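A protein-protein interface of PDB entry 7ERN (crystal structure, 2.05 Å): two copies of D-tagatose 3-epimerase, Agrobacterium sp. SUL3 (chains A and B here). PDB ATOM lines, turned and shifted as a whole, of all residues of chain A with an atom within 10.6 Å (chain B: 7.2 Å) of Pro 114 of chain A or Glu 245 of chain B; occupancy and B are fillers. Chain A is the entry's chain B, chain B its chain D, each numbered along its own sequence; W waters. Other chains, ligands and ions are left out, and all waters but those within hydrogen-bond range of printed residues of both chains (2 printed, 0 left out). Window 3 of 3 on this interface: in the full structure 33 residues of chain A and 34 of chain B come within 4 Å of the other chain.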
ATOM      1  N   SER A  74     -11.659   2.956 -24.901  1.00  0.00           N
ATOM      2  CA  SER A  74     -11.909   3.858 -23.781  1.00  0.00           C
ATOM      3  C   SER A  74     -12.350   3.098 -22.534  1.00  0.00           C
ATOM      4  O   SER A  74     -12.084   3.545 -21.410  1.00  0.00           O
ATOM      5  CB  SER A  74     -12.952   4.911 -24.168  1.00  0.00           C
ATOM      6  OG  SER A  74     -14.273   4.379 -24.165  1.00  0.00           O
ATOM      7  N   GLU A 109     -19.958   5.654 -30.858  1.00  0.00           N
ATOM      8  CA  GLU A 109     -19.516   5.622 -29.476  1.00  0.00           C
ATOM      9  C   GLU A 109     -19.854   6.938 -28.802  1.00  0.00           C
ATOM     10  O   GLU A 109     -19.510   8.016 -29.300  1.00  0.00           O
ATOM     11  CB  GLU A 109     -18.012   5.358 -29.376  1.00  0.00           C
ATOM     12  CG  GLU A 109     -17.492   5.472 -27.947  1.00  0.00           C
ATOM     13  CD  GLU A 109     -16.107   4.886 -27.755  1.00  0.00           C
ATOM     14  OE1 GLU A 109     -15.759   4.574 -26.596  1.00  0.00           O
ATOM     15  OE2 GLU A 109     -15.356   4.760 -28.752  1.00  0.00           O
ATOM     16  N   ARG A 110     -20.521   6.847 -27.665  1.00  0.00           N
ATOM     17  CA  ARG A 110     -20.734   8.034 -26.863  1.00  0.00           C
ATOM     18  C   ARG A 110     -21.022   7.581 -25.448  1.00  0.00           C
ATOM     19  O   ARG A 110     -21.486   6.463 -25.206  1.00  0.00           O
ATOM     20  CB  ARG A 110     -21.878   8.897 -27.398  1.00  0.00           C
ATOM     21  CG  ARG A 110     -23.191   8.130 -27.520  1.00  0.00           C
ATOM     22  CD  ARG A 110     -24.334   8.952 -26.974  1.00  0.00           C
ATOM     23  NE  ARG A 110     -24.449  10.214 -27.687  1.00  0.00           N
ATOM     24  CZ  ARG A 110     -24.904  11.333 -27.141  1.00  0.00           C
ATOM     25  NH1 ARG A 110     -25.290  11.349 -25.869  1.00  0.00           N
ATOM     26  NH2 ARG A 110     -24.969  12.435 -27.869  1.00  0.00           N
ATOM     27  N   THR A 111     -20.735   8.474 -24.524  1.00  0.00           N
ATOM     28  CA  THR A 111     -20.921   8.212 -23.122  1.00  0.00           C
ATOM     29  C   THR A 111     -22.010   9.084 -22.514  1.00  0.00           C
ATOM     30  O   THR A 111     -22.493   8.777 -21.421  1.00  0.00           O
ATOM     31  CB  THR A 111     -19.585   8.435 -22.408  1.00  0.00           C
ATOM     32  OG1 THR A 111     -19.536   7.661 -21.216  1.00  0.00           O
ATOM     33  CG2 THR A 111     -19.403   9.885 -22.083  1.00  0.00           C
ATOM     34  N   GLY A 112     -22.432  10.139 -23.214  1.00  0.00           N
ATOM     35  CA  GLY A 112     -23.320  11.137 -22.666  1.00  0.00           C
ATOM     36  C   GLY A 112     -22.623  12.323 -22.038  1.00  0.00           C
ATOM     37  O   GLY A 112     -23.284  13.326 -21.752  1.00  0.00           O
ATOM     38  N   PHE A 113     -21.317  12.243 -21.827  1.00  0.00           N
ATOM     39  CA  PHE A 113     -20.508  13.248 -21.158  1.00  0.00           C
ATOM     40  C   PHE A 113     -19.268  13.566 -21.980  1.00  0.00           C
ATOM     41  O   PHE A 113     -18.917  12.825 -22.905  1.00  0.00           O
ATOM     42  CB  PHE A 113     -20.105  12.748 -19.766  1.00  0.00           C
ATOM     43  CG  PHE A 113     -21.275  12.264 -18.947  1.00  0.00           C
ATOM     44  CD1 PHE A 113     -22.053  13.159 -18.229  1.00  0.00           C
ATOM     45  CD2 PHE A 113     -21.616  10.923 -18.926  1.00  0.00           C
ATOM     46  CE1 PHE A 113     -23.134  12.727 -17.487  1.00  0.00           C
ATOM     47  CE2 PHE A 113     -22.703  10.481 -18.189  1.00  0.00           C
ATOM     48  CZ  PHE A 113     -23.461  11.386 -17.466  1.00  0.00           C
ATOM     49  N   PRO A 114     -18.599  14.681 -21.690  1.00  0.00           N
ATOM     50  CA  PRO A 114     -17.297  14.949 -22.313  1.00  0.00           C
ATOM     51  C   PRO A 114     -16.298  13.860 -21.970  1.00  0.00           C
ATOM     52  O   PRO A 114     -16.431  13.181 -20.936  1.00  0.00           O
ATOM     53  CB  PRO A 114     -16.882  16.297 -21.702  1.00  0.00           C
ATOM     54  CG  PRO A 114     -18.165  16.964 -21.364  1.00  0.00           C
ATOM     55  CD  PRO A 114     -19.113  15.853 -20.955  1.00  0.00           C
ATOM     56  N   PRO A 115     -15.272  13.674 -22.801  1.00  0.00           N
ATOM     57  CA  PRO A 115     -14.290  12.615 -22.531  1.00  0.00           C
ATOM     58  C   PRO A 115     -13.468  12.922 -21.285  1.00  0.00           C
ATOM     59  O   PRO A 115     -13.065  14.062 -21.051  1.00  0.00           O
ATOM     60  CB  PRO A 115     -13.419  12.611 -23.792  1.00  0.00           C
ATOM     61  CG  PRO A 115     -13.513  14.031 -24.302  1.00  0.00           C
ATOM     62  CD  PRO A 115     -14.919  14.472 -23.991  1.00  0.00           C
ATOM     63  N   THR A 116     -13.226  11.890 -20.485  1.00  0.00           N
ATOM     64  CA  THR A 116     -12.505  12.019 -19.226  1.00  0.00           C
ATOM     65  C   THR A 116     -11.032  11.679 -19.414  1.00  0.00           C
ATOM     66  O   THR A 116     -10.635  11.025 -20.382  1.00  0.00           O
ATOM     67  CB  THR A 116     -13.093  11.095 -18.159  1.00  0.00           C
ATOM     68  OG1 THR A 116     -12.792   9.736 -18.499  1.00  0.00           O
ATOM     69  CG2 THR A 116     -14.620  11.265 -18.062  1.00  0.00           C
ATOM     70  N   GLN A 117     -10.220  12.126 -18.454  1.00  0.00           N
ATOM     71  CA  GLN A 117      -8.812  11.754 -18.472  1.00  0.00           C
ATOM     72  C   GLN A 117      -8.642  10.246 -18.336  1.00  0.00           C
ATOM     73  O   GLN A 117      -7.714   9.667 -18.915  1.00  0.00           O
ATOM     74  CB  GLN A 117      -8.062  12.494 -17.364  1.00  0.00           C
ATOM     75  CG  GLN A 117      -6.559  12.244 -17.354  1.00  0.00           C
ATOM     76  CD  GLN A 117      -5.883  12.705 -18.636  1.00  0.00           C
ATOM     77  OE1 GLN A 117      -5.767  13.906 -18.906  1.00  0.00           O
ATOM     78  NE2 GLN A 117      -5.437  11.745 -19.436  1.00  0.00           N
ATOM     79  N   ALA A 118      -9.542   9.590 -17.607  1.00  0.00           N
ATOM     80  CA  ALA A 118      -9.417   8.153 -17.415  1.00  0.00           C
ATOM     81  C   ALA A 118      -9.608   7.415 -18.735  1.00  0.00           C
ATOM     82  O   ALA A 118      -8.907   6.433 -19.020  1.00  0.00           O
ATOM     83  CB  ALA A 118     -10.424   7.689 -16.372  1.00  0.00           C
ATOM     84  N   GLU A 119     -10.541   7.894 -19.560  1.00  0.00           N
ATOM     85  CA  GLU A 119     -10.726   7.328 -20.888  1.00  0.00           C
ATOM     86  C   GLU A 119      -9.482   7.513 -21.740  1.00  0.00           C
ATOM     87  O   GLU A 119      -9.062   6.585 -22.445  1.00  0.00           O
ATOM     88  CB  GLU A 119     -11.935   7.971 -21.563  1.00  0.00           C
ATOM     89  CG  GLU A 119     -13.274   7.417 -21.072  1.00  0.00           C
ATOM     90  CD  GLU A 119     -14.459   8.214 -21.595  1.00  0.00           C
ATOM     91  OE1 GLU A 119     -14.504   9.443 -21.353  1.00  0.00           O
ATOM     92  OE2 GLU A 119     -15.336   7.613 -22.259  1.00  0.00           O
ATOM     93  N   TYR A 120      -8.875   8.711 -21.691  1.00  0.00           N
ATOM     94  CA  TYR A 120      -7.687   8.961 -22.496  1.00  0.00           C
ATOM     95  C   TYR A 120      -6.498   8.145 -22.002  1.00  0.00           C
ATOM     96  O   TYR A 120      -5.646   7.744 -22.810  1.00  0.00           O
ATOM     97  CB  TYR A 120      -7.351  10.459 -22.510  1.00  0.00           C
ATOM     98  CG  TYR A 120      -8.252  11.289 -23.417  1.00  0.00           C
ATOM     99  CD1 TYR A 120      -8.292  11.059 -24.792  1.00  0.00           C
ATOM    100  CD2 TYR A 120      -9.058  12.294 -22.896  1.00  0.00           C
ATOM    101  CE1 TYR A 120      -9.121  11.808 -25.624  1.00  0.00           C
ATOM    102  CE2 TYR A 120      -9.894  13.055 -23.725  1.00  0.00           C
ATOM    103  CZ  TYR A 120      -9.916  12.805 -25.084  1.00  0.00           C
ATOM    104  OH  TYR A 120     -10.730  13.543 -25.902  1.00  0.00           O
ATOM    105  N   ARG A 148     -18.319  14.792 -33.856  1.00  0.00           N
ATOM    106  CA  ARG A 148     -18.867  14.661 -32.509  1.00  0.00           C
ATOM    107  C   ARG A 148     -20.007  13.653 -32.420  1.00  0.00           C
ATOM    108  O   ARG A 148     -20.299  13.161 -31.322  1.00  0.00           O
ATOM    109  CB  ARG A 148     -19.372  16.022 -32.041  1.00  0.00           C
ATOM    110  CG  ARG A 148     -20.453  16.596 -32.967  1.00  0.00           C
ATOM    111  CD  ARG A 148     -20.518  18.105 -32.884  1.00  0.00           C
ATOM    112  NE  ARG A 148     -19.209  18.697 -33.120  1.00  0.00           N
ATOM    113  CZ  ARG A 148     -18.930  19.982 -32.939  1.00  0.00           C
ATOM    114  NH1 ARG A 148     -19.877  20.815 -32.517  1.00  0.00           N
ATOM    115  NH2 ARG A 148     -17.704  20.426 -33.181  1.00  0.00           N
ATOM    116  N   ASN A 151     -18.215   9.826 -32.250  1.00  0.00           N
ATOM    117  CA  ASN A 151     -17.288   9.485 -31.189  1.00  0.00           C
ATOM    118  C   ASN A 151     -17.047  10.742 -30.364  1.00  0.00           C
ATOM    119  O   ASN A 151     -17.006  11.844 -30.912  1.00  0.00           O
ATOM    120  CB  ASN A 151     -15.987   8.960 -31.804  1.00  0.00           C
ATOM    121  CG  ASN A 151     -15.005   8.518 -30.776  1.00  0.00           C
ATOM    122  OD1 ASN A 151     -14.204   9.316 -30.285  1.00  0.00           O
ATOM    123  ND2 ASN A 151     -15.048   7.236 -30.437  1.00  0.00           N
ATOM    124  N   HIS A 152     -16.885  10.584 -29.058  1.00  0.00           N
ATOM    125  CA  HIS A 152     -16.731  11.738 -28.176  1.00  0.00           C
ATOM    126  C   HIS A 152     -15.290  11.996 -27.763  1.00  0.00           C
ATOM    127  O   HIS A 152     -15.042  12.901 -26.958  1.00  0.00           O
ATOM    128  CB  HIS A 152     -17.574  11.552 -26.917  1.00  0.00           C
ATOM    129  CG  HIS A 152     -17.089  10.439 -26.040  1.00  0.00           C
ATOM    130  ND1 HIS A 152     -17.039   9.128 -26.463  1.00  0.00           N
ATOM    131  CD2 HIS A 152     -16.628  10.443 -24.765  1.00  0.00           C
ATOM    132  CE1 HIS A 152     -16.573   8.370 -25.486  1.00  0.00           C
ATOM    133  NE2 HIS A 152     -16.315   9.143 -24.445  1.00  0.00           N
ATOM    134  N   LEU A 153     -14.338  11.229 -28.283  1.00  0.00           N
ATOM    135  CA  LEU A 153     -12.973  11.238 -27.771  1.00  0.00           C
ATOM    136  C   LEU A 153     -11.976  11.965 -28.660  1.00  0.00           C
ATOM    137  O   LEU A 153     -11.119  12.686 -28.150  1.00  0.00           O
ATOM    138  CB  LEU A 153     -12.491   9.799 -27.559  1.00  0.00           C
ATOM    139  CG  LEU A 153     -13.246   8.957 -26.531  1.00  0.00           C
ATOM    140  CD1 LEU A 153     -13.154   7.492 -26.938  1.00  0.00           C
ATOM    141  CD2 LEU A 153     -12.653   9.167 -25.143  1.00  0.00           C
ATOM    142  N   VAL A 154     -12.029  11.781 -29.976  1.00  0.00           N
ATOM    143  CA  VAL A 154     -11.043  12.366 -30.888  1.00  0.00           C
ATOM    144  C   VAL A 154     -11.819  12.986 -32.047  1.00  0.00           C
ATOM    145  O   VAL A 154     -12.091  12.326 -33.055  1.00  0.00           O
ATOM    146  CB  VAL A 154     -10.015  11.344 -31.390  1.00  0.00           C
ATOM    147  CG1 VAL A 154      -9.017  12.017 -32.306  1.00  0.00           C
ATOM    148  CG2 VAL A 154      -9.303  10.661 -30.218  1.00  0.00           C
ATOM    149  N   ASN A 155     -12.152  14.274 -31.927  1.00  0.00           N
ATOM    150  CA  ASN A 155     -12.907  14.991 -32.947  1.00  0.00           C
ATOM    151  C   ASN A 155     -12.085  15.998 -33.736  1.00  0.00           C
ATOM    152  O   ASN A 155     -12.241  16.086 -34.956  1.00  0.00           O
ATOM    153  CB  ASN A 155     -14.097  15.712 -32.311  1.00  0.00           C
ATOM    154  CG  ASN A 155     -15.038  14.759 -31.604  1.00  0.00           C
ATOM    155  OD1 ASN A 155     -15.662  15.122 -30.618  1.00  0.00           O
ATOM    156  ND2 ASN A 155     -15.140  13.534 -32.109  1.00  0.00           N
ATOM    157  N   GLN A 159      -7.049  17.494 -30.805  1.00  0.00           N
ATOM    158  CA  GLN A 159      -7.200  16.335 -29.935  1.00  0.00           C
ATOM    159  C   GLN A 159      -6.363  15.170 -30.426  1.00  0.00           C
ATOM    160  O   GLN A 159      -5.727  14.481 -29.622  1.00  0.00           O
ATOM    161  CB  GLN A 159      -8.672  15.926 -29.842  1.00  0.00           C
ATOM    162  CG  GLN A 159      -9.517  16.915 -29.055  1.00  0.00           C
ATOM    163  CD  GLN A 159     -10.990  16.536 -29.047  1.00  0.00           C
ATOM    164  OE1 GLN A 159     -11.586  16.305 -30.095  1.00  0.00           O
ATOM    165  NE2 GLN A 159     -11.577  16.459 -27.862  1.00  0.00           N
ATOM    166  N   ALA B 242     -23.031  29.458 -25.110  1.00  0.00           N
ATOM    167  CA  ALA B 242     -23.446  29.635 -23.723  1.00  0.00           C
ATOM    168  C   ALA B 242     -23.880  28.336 -23.055  1.00  0.00           C
ATOM    169  O   ALA B 242     -24.270  28.363 -21.883  1.00  0.00           O
ATOM    170  CB  ALA B 242     -24.584  30.661 -23.629  1.00  0.00           C
ATOM    171  N   MET B 243     -23.811  27.212 -23.763  1.00  0.00           N
ATOM    172  CA  MET B 243     -24.364  25.954 -23.253  1.00  0.00           C
ATOM    173  C   MET B 243     -23.571  25.444 -22.052  1.00  0.00           C
ATOM    174  O   MET B 243     -22.339  25.334 -22.129  1.00  0.00           O
ATOM    175  CB  MET B 243     -24.361  24.897 -24.349  1.00  0.00           C
ATOM    176  CG  MET B 243     -25.361  25.162 -25.433  1.00  0.00           C
ATOM    177  SD  MET B 243     -26.995  24.558 -24.992  1.00  0.00           S
ATOM    178  CE  MET B 243     -27.752  24.525 -26.616  1.00  0.00           C
ATOM    179  N   PRO B 244     -24.236  25.093 -20.948  1.00  0.00           N
ATOM    180  CA  PRO B 244     -23.517  24.528 -19.800  1.00  0.00           C
ATOM    181  C   PRO B 244     -23.006  23.127 -20.099  1.00  0.00           C
ATOM    182  O   PRO B 244     -23.561  22.402 -20.927  1.00  0.00           O
ATOM    183  CB  PRO B 244     -24.575  24.508 -18.692  1.00  0.00           C
ATOM    184  CG  PRO B 244     -25.884  24.447 -19.419  1.00  0.00           C
ATOM    185  CD  PRO B 244     -25.685  25.212 -20.702  1.00  0.00           C
ATOM    186  N   GLU B 245     -21.926  22.753 -19.400  1.00  0.00           N
ATOM    187  CA  GLU B 245     -21.284  21.461 -19.636  1.00  0.00           C
ATOM    188  C   GLU B 245     -22.243  20.292 -19.416  1.00  0.00           C
ATOM    189  O   GLU B 245     -22.083  19.233 -20.033  1.00  0.00           O
ATOM    190  CB  GLU B 245     -20.053  21.324 -18.739  1.00  0.00           C
ATOM    191  CG  GLU B 245     -19.317  20.005 -18.894  1.00  0.00           C
ATOM    192  CD  GLU B 245     -17.893  20.049 -18.371  1.00  0.00           C
ATOM    193  OE1 GLU B 245     -17.394  21.163 -18.088  1.00  0.00           O
ATOM    194  OE2 GLU B 245     -17.278  18.963 -18.245  1.00  0.00           O
ATOM    195  N   GLU B 246     -23.249  20.465 -18.555  1.00  0.00           N
ATOM    196  CA  GLU B 246     -24.222  19.408 -18.308  1.00  0.00           C
ATOM    197  C   GLU B 246     -25.133  19.155 -19.508  1.00  0.00           C
ATOM    198  O   GLU B 246     -25.793  18.111 -19.563  1.00  0.00           O
ATOM    199  CB  GLU B 246     -25.062  19.756 -17.075  1.00  0.00           C
ATOM    200  CG  GLU B 246     -24.243  20.194 -15.865  1.00  0.00           C
ATOM    201  CD  GLU B 246     -23.927  21.687 -15.865  1.00  0.00           C
ATOM    202  OE1 GLU B 246     -22.832  22.071 -15.391  1.00  0.00           O
ATOM    203  OE2 GLU B 246     -24.777  22.473 -16.337  1.00  0.00           O
ATOM    204  N   MET B 247     -25.190  20.081 -20.463  1.00  0.00           N
ATOM    205  CA  MET B 247     -26.024  19.900 -21.643  1.00  0.00           C
ATOM    206  C   MET B 247     -25.367  19.024 -22.700  1.00  0.00           C
ATOM    207  O   MET B 247     -26.033  18.676 -23.679  1.00  0.00           O
ATOM    208  CB  MET B 247     -26.366  21.263 -22.246  1.00  0.00           C
ATOM    209  CG  MET B 247     -27.593  21.912 -21.639  1.00  0.00           C
ATOM    210  SD  MET B 247     -29.089  21.018 -22.090  1.00  0.00           S
ATOM    211  CE  MET B 247     -29.079  21.238 -23.873  1.00  0.00           C
ATOM    212  N   ALA B 248     -24.097  18.649 -22.494  1.00  0.00           N
ATOM    213  CA  ALA B 248     -23.278  17.991 -23.515  1.00  0.00           C
ATOM    214  C   ALA B 248     -24.000  16.832 -24.203  1.00  0.00           C
ATOM    215  O   ALA B 248     -24.029  16.751 -25.438  1.00  0.00           O
ATOM    216  CB  ALA B 248     -21.973  17.498 -22.880  1.00  0.00           C
ATOM    217  N   GLY B 249     -24.570  15.910 -23.418  1.00  0.00           N
ATOM    218  CA  GLY B 249     -25.181  14.721 -24.004  1.00  0.00           C
ATOM    219  C   GLY B 249     -26.369  15.030 -24.896  1.00  0.00           C
ATOM    220  O   GLY B 249     -26.586  14.364 -25.913  1.00  0.00           O
ATOM    221  N   THR B 253     -22.279  17.687 -27.893  1.00  0.00           N
ATOM    222  CA  THR B 253     -21.192  18.666 -27.911  1.00  0.00           C
ATOM    223  C   THR B 253     -20.267  18.336 -26.747  1.00  0.00           C
ATOM    224  O   THR B 253     -20.712  18.306 -25.596  1.00  0.00           O
ATOM    225  CB  THR B 253     -21.738  20.090 -27.794  1.00  0.00           C
ATOM    226  OG1 THR B 253     -22.745  20.284 -28.798  1.00  0.00           O
ATOM    227  CG2 THR B 253     -20.639  21.106 -27.997  1.00  0.00           C
ATOM    228  N   TRP B 254     -18.994  18.064 -27.047  1.00  0.00           N
ATOM    229  CA  TRP B 254     -18.058  17.520 -26.068  1.00  0.00           C
ATOM    230  C   TRP B 254     -16.946  18.491 -25.671  1.00  0.00           C
ATOM    231  O   TRP B 254     -16.138  18.158 -24.794  1.00  0.00           O
ATOM    232  CB  TRP B 254     -17.438  16.224 -26.603  1.00  0.00           C
ATOM    233  CG  TRP B 254     -18.445  15.305 -27.218  1.00  0.00           C
ATOM    234  CD1 TRP B 254     -18.440  14.811 -28.495  1.00  0.00           C
ATOM    235  CD2 TRP B 254     -19.625  14.788 -26.591  1.00  0.00           C
ATOM    236  NE1 TRP B 254     -19.545  14.005 -28.693  1.00  0.00           N
ATOM    237  CE2 TRP B 254     -20.284  13.976 -27.541  1.00  0.00           C
ATOM    238  CE3 TRP B 254     -20.183  14.920 -25.312  1.00  0.00           C
ATOM    239  CZ2 TRP B 254     -21.476  13.298 -27.252  1.00  0.00           C
ATOM    240  CZ3 TRP B 254     -21.370  14.251 -25.032  1.00  0.00           C
ATOM    241  CH2 TRP B 254     -22.003  13.454 -25.997  1.00  0.00           C
ATOM    242  N   ARG B 255     -16.890  19.676 -26.272  1.00  0.00           N
ATOM    243  CA  ARG B 255     -15.852  20.657 -25.979  1.00  0.00           C
ATOM    244  C   ARG B 255     -16.399  22.043 -26.309  1.00  0.00           C
ATOM    245  O   ARG B 255     -17.408  22.160 -27.017  1.00  0.00           O
ATOM    246  CB  ARG B 255     -14.575  20.364 -26.786  1.00  0.00           C
ATOM    247  CG  ARG B 255     -14.794  20.350 -28.291  1.00  0.00           C
ATOM    248  CD  ARG B 255     -13.600  19.753 -29.013  1.00  0.00           C
ATOM    249  NE  ARG B 255     -13.928  19.570 -30.421  1.00  0.00           N
ATOM    250  CZ  ARG B 255     -13.633  20.451 -31.362  1.00  0.00           C
ATOM    251  NH1 ARG B 255     -12.975  21.556 -31.026  1.00  0.00           N
ATOM    252  NH2 ARG B 255     -13.982  20.221 -32.625  1.00  0.00           N
HETATM  253  O   HOH W   1     -22.349  20.671 -31.583  1.00  0.00           O
HETATM  254  O   HOH W   2     -16.130  17.866 -30.956  1.00  0.00           O
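The guanidinium group (NH2) of Arg 110 of chain A lies within hydrogen-bond range of the backbone carbonyl oxygen (O) of Gly 249 of chain B, 3.2 Å away. The backbone carbonyl oxygen of Gly 112 of chain A sits close to the backbone NH of Gly 249 of chain B (3.3 Å). The indole nitrogen (NE1) of Trp 254 of chain B sits at hydrogen-bond distance from the backbone carbonyl oxygen (O) of Arg 148 of chain A, 2.9 Å away.
No position is printed for both chains. Of the 13 pairs that touch across the chains among the printed residues, none has its exchanged pair printed and touching as well.
Printed residues of chain A that touch a printed residue of chain B: Arg 110, Gly 112, Phe 113, Pro 114, Pro 115, Arg 148, His 152 and Asn 155. Of the 11 printed residues of chain B, 5 touch a printed residue of chain A. Printed residues of chain B that touch a printed residue of chain A: Glu 245, Ala 248, Gly 249, Trp 254 and Arg 255. Hydrophobic or aromatic side chains of chain B that line the printed part of chain A: Ala 248 and Trp 254. Among the printed residues, 13 pairs touch across the chains.
Trp 254 of chain B touches Arg 110 of chain A (CZ2 to NH2, 3.7 Å). Trp 254 of chain B touches Gly 112 of chain A. Trp 254 of chain B touches Phe 113 of chain A. CG of Pro 114 of chain A touches OE2 of Glu 245 of chain B, 3.8 Å away. Pro 114 of chain A touches Ala 248 of chain B. Trp 254 of chain B touches Pro 114 of chain A (O to CB, 3.7 Å). O of Trp 254 of chain B touches CD of Pro 115 of chain A, at 3.96 Å. Arg 148 of chain A touches Arg 255 of chain B. CA of His 152 of chain A touches CD1 of Trp 254 of chain B (3.5 Å). Asn 155 of chain A touches Trp 254 of chain B.
Pro 114 of chain A touches three residues of chain B. Of the printed residues of chain A, Glu 245 of chain B touches Pro 114 (3.8 Å). No residue of chain A comes within 4 Å of Pro 244 of chain B. No residue of chain A comes within 4 Å of Glu 246 of chain B. Ala 248 of chain B touches just one residue of chain A: Pro 114. Of the printed residues of chain B, His 152 of chain A touches Trp 254. Printed residues of chain B within 4 Å of Arg 148 of chain A: Trp 254 and Arg 255. Printed residues of chain A within 4 Å of Gly 249 of chain B: Arg 110 (3.2 Å) and Gly 112 (3.3 Å). Printed residues of chain B within 4 Å of Arg 110 of chain A: Gly 249 (3.2 Å) and Trp 254 (3.7 Å). Gln 159 of chain A touches none of the printed residues of chain B. Met 247 of chain B touches none of the printed residues of chain A. The nearest printed residue of chain A that does not touch Arg 255 of chain B is Gln 159 of chain A (4.03 Å).
NE2 of His 152 of chain A sits at hydrogen-bond distance from OE2 of Glu 119 of chain A. The backbone carbonyl oxygen (O) of Asn 151 of chain A lies within hydrogen-bond range of the side-chain amide nitrogen (ND2) of Asn 155 of chain A. The backbone NH (N) of Asn 155 of chain A sits at hydrogen-bond distance from the side-chain amide oxygen (OE1) of Gln 159 of chain A (2.8 Å). The backbone NH (N) of Thr 253 of chain B is in hydrogen-bond range of the backbone carbonyl oxygen (O) of Ala 248 of chain B.
Water W1 bridges NH1 of Arg 148 of chain A (2.6 Å) and OG1 of Thr 253 of chain B (2.8 Å). Water W2 lies within hydrogen-bond range of OD1 of Asn 155 of chain A (2.8 Å) and NE of Arg 255 of chain B (2.8 Å).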
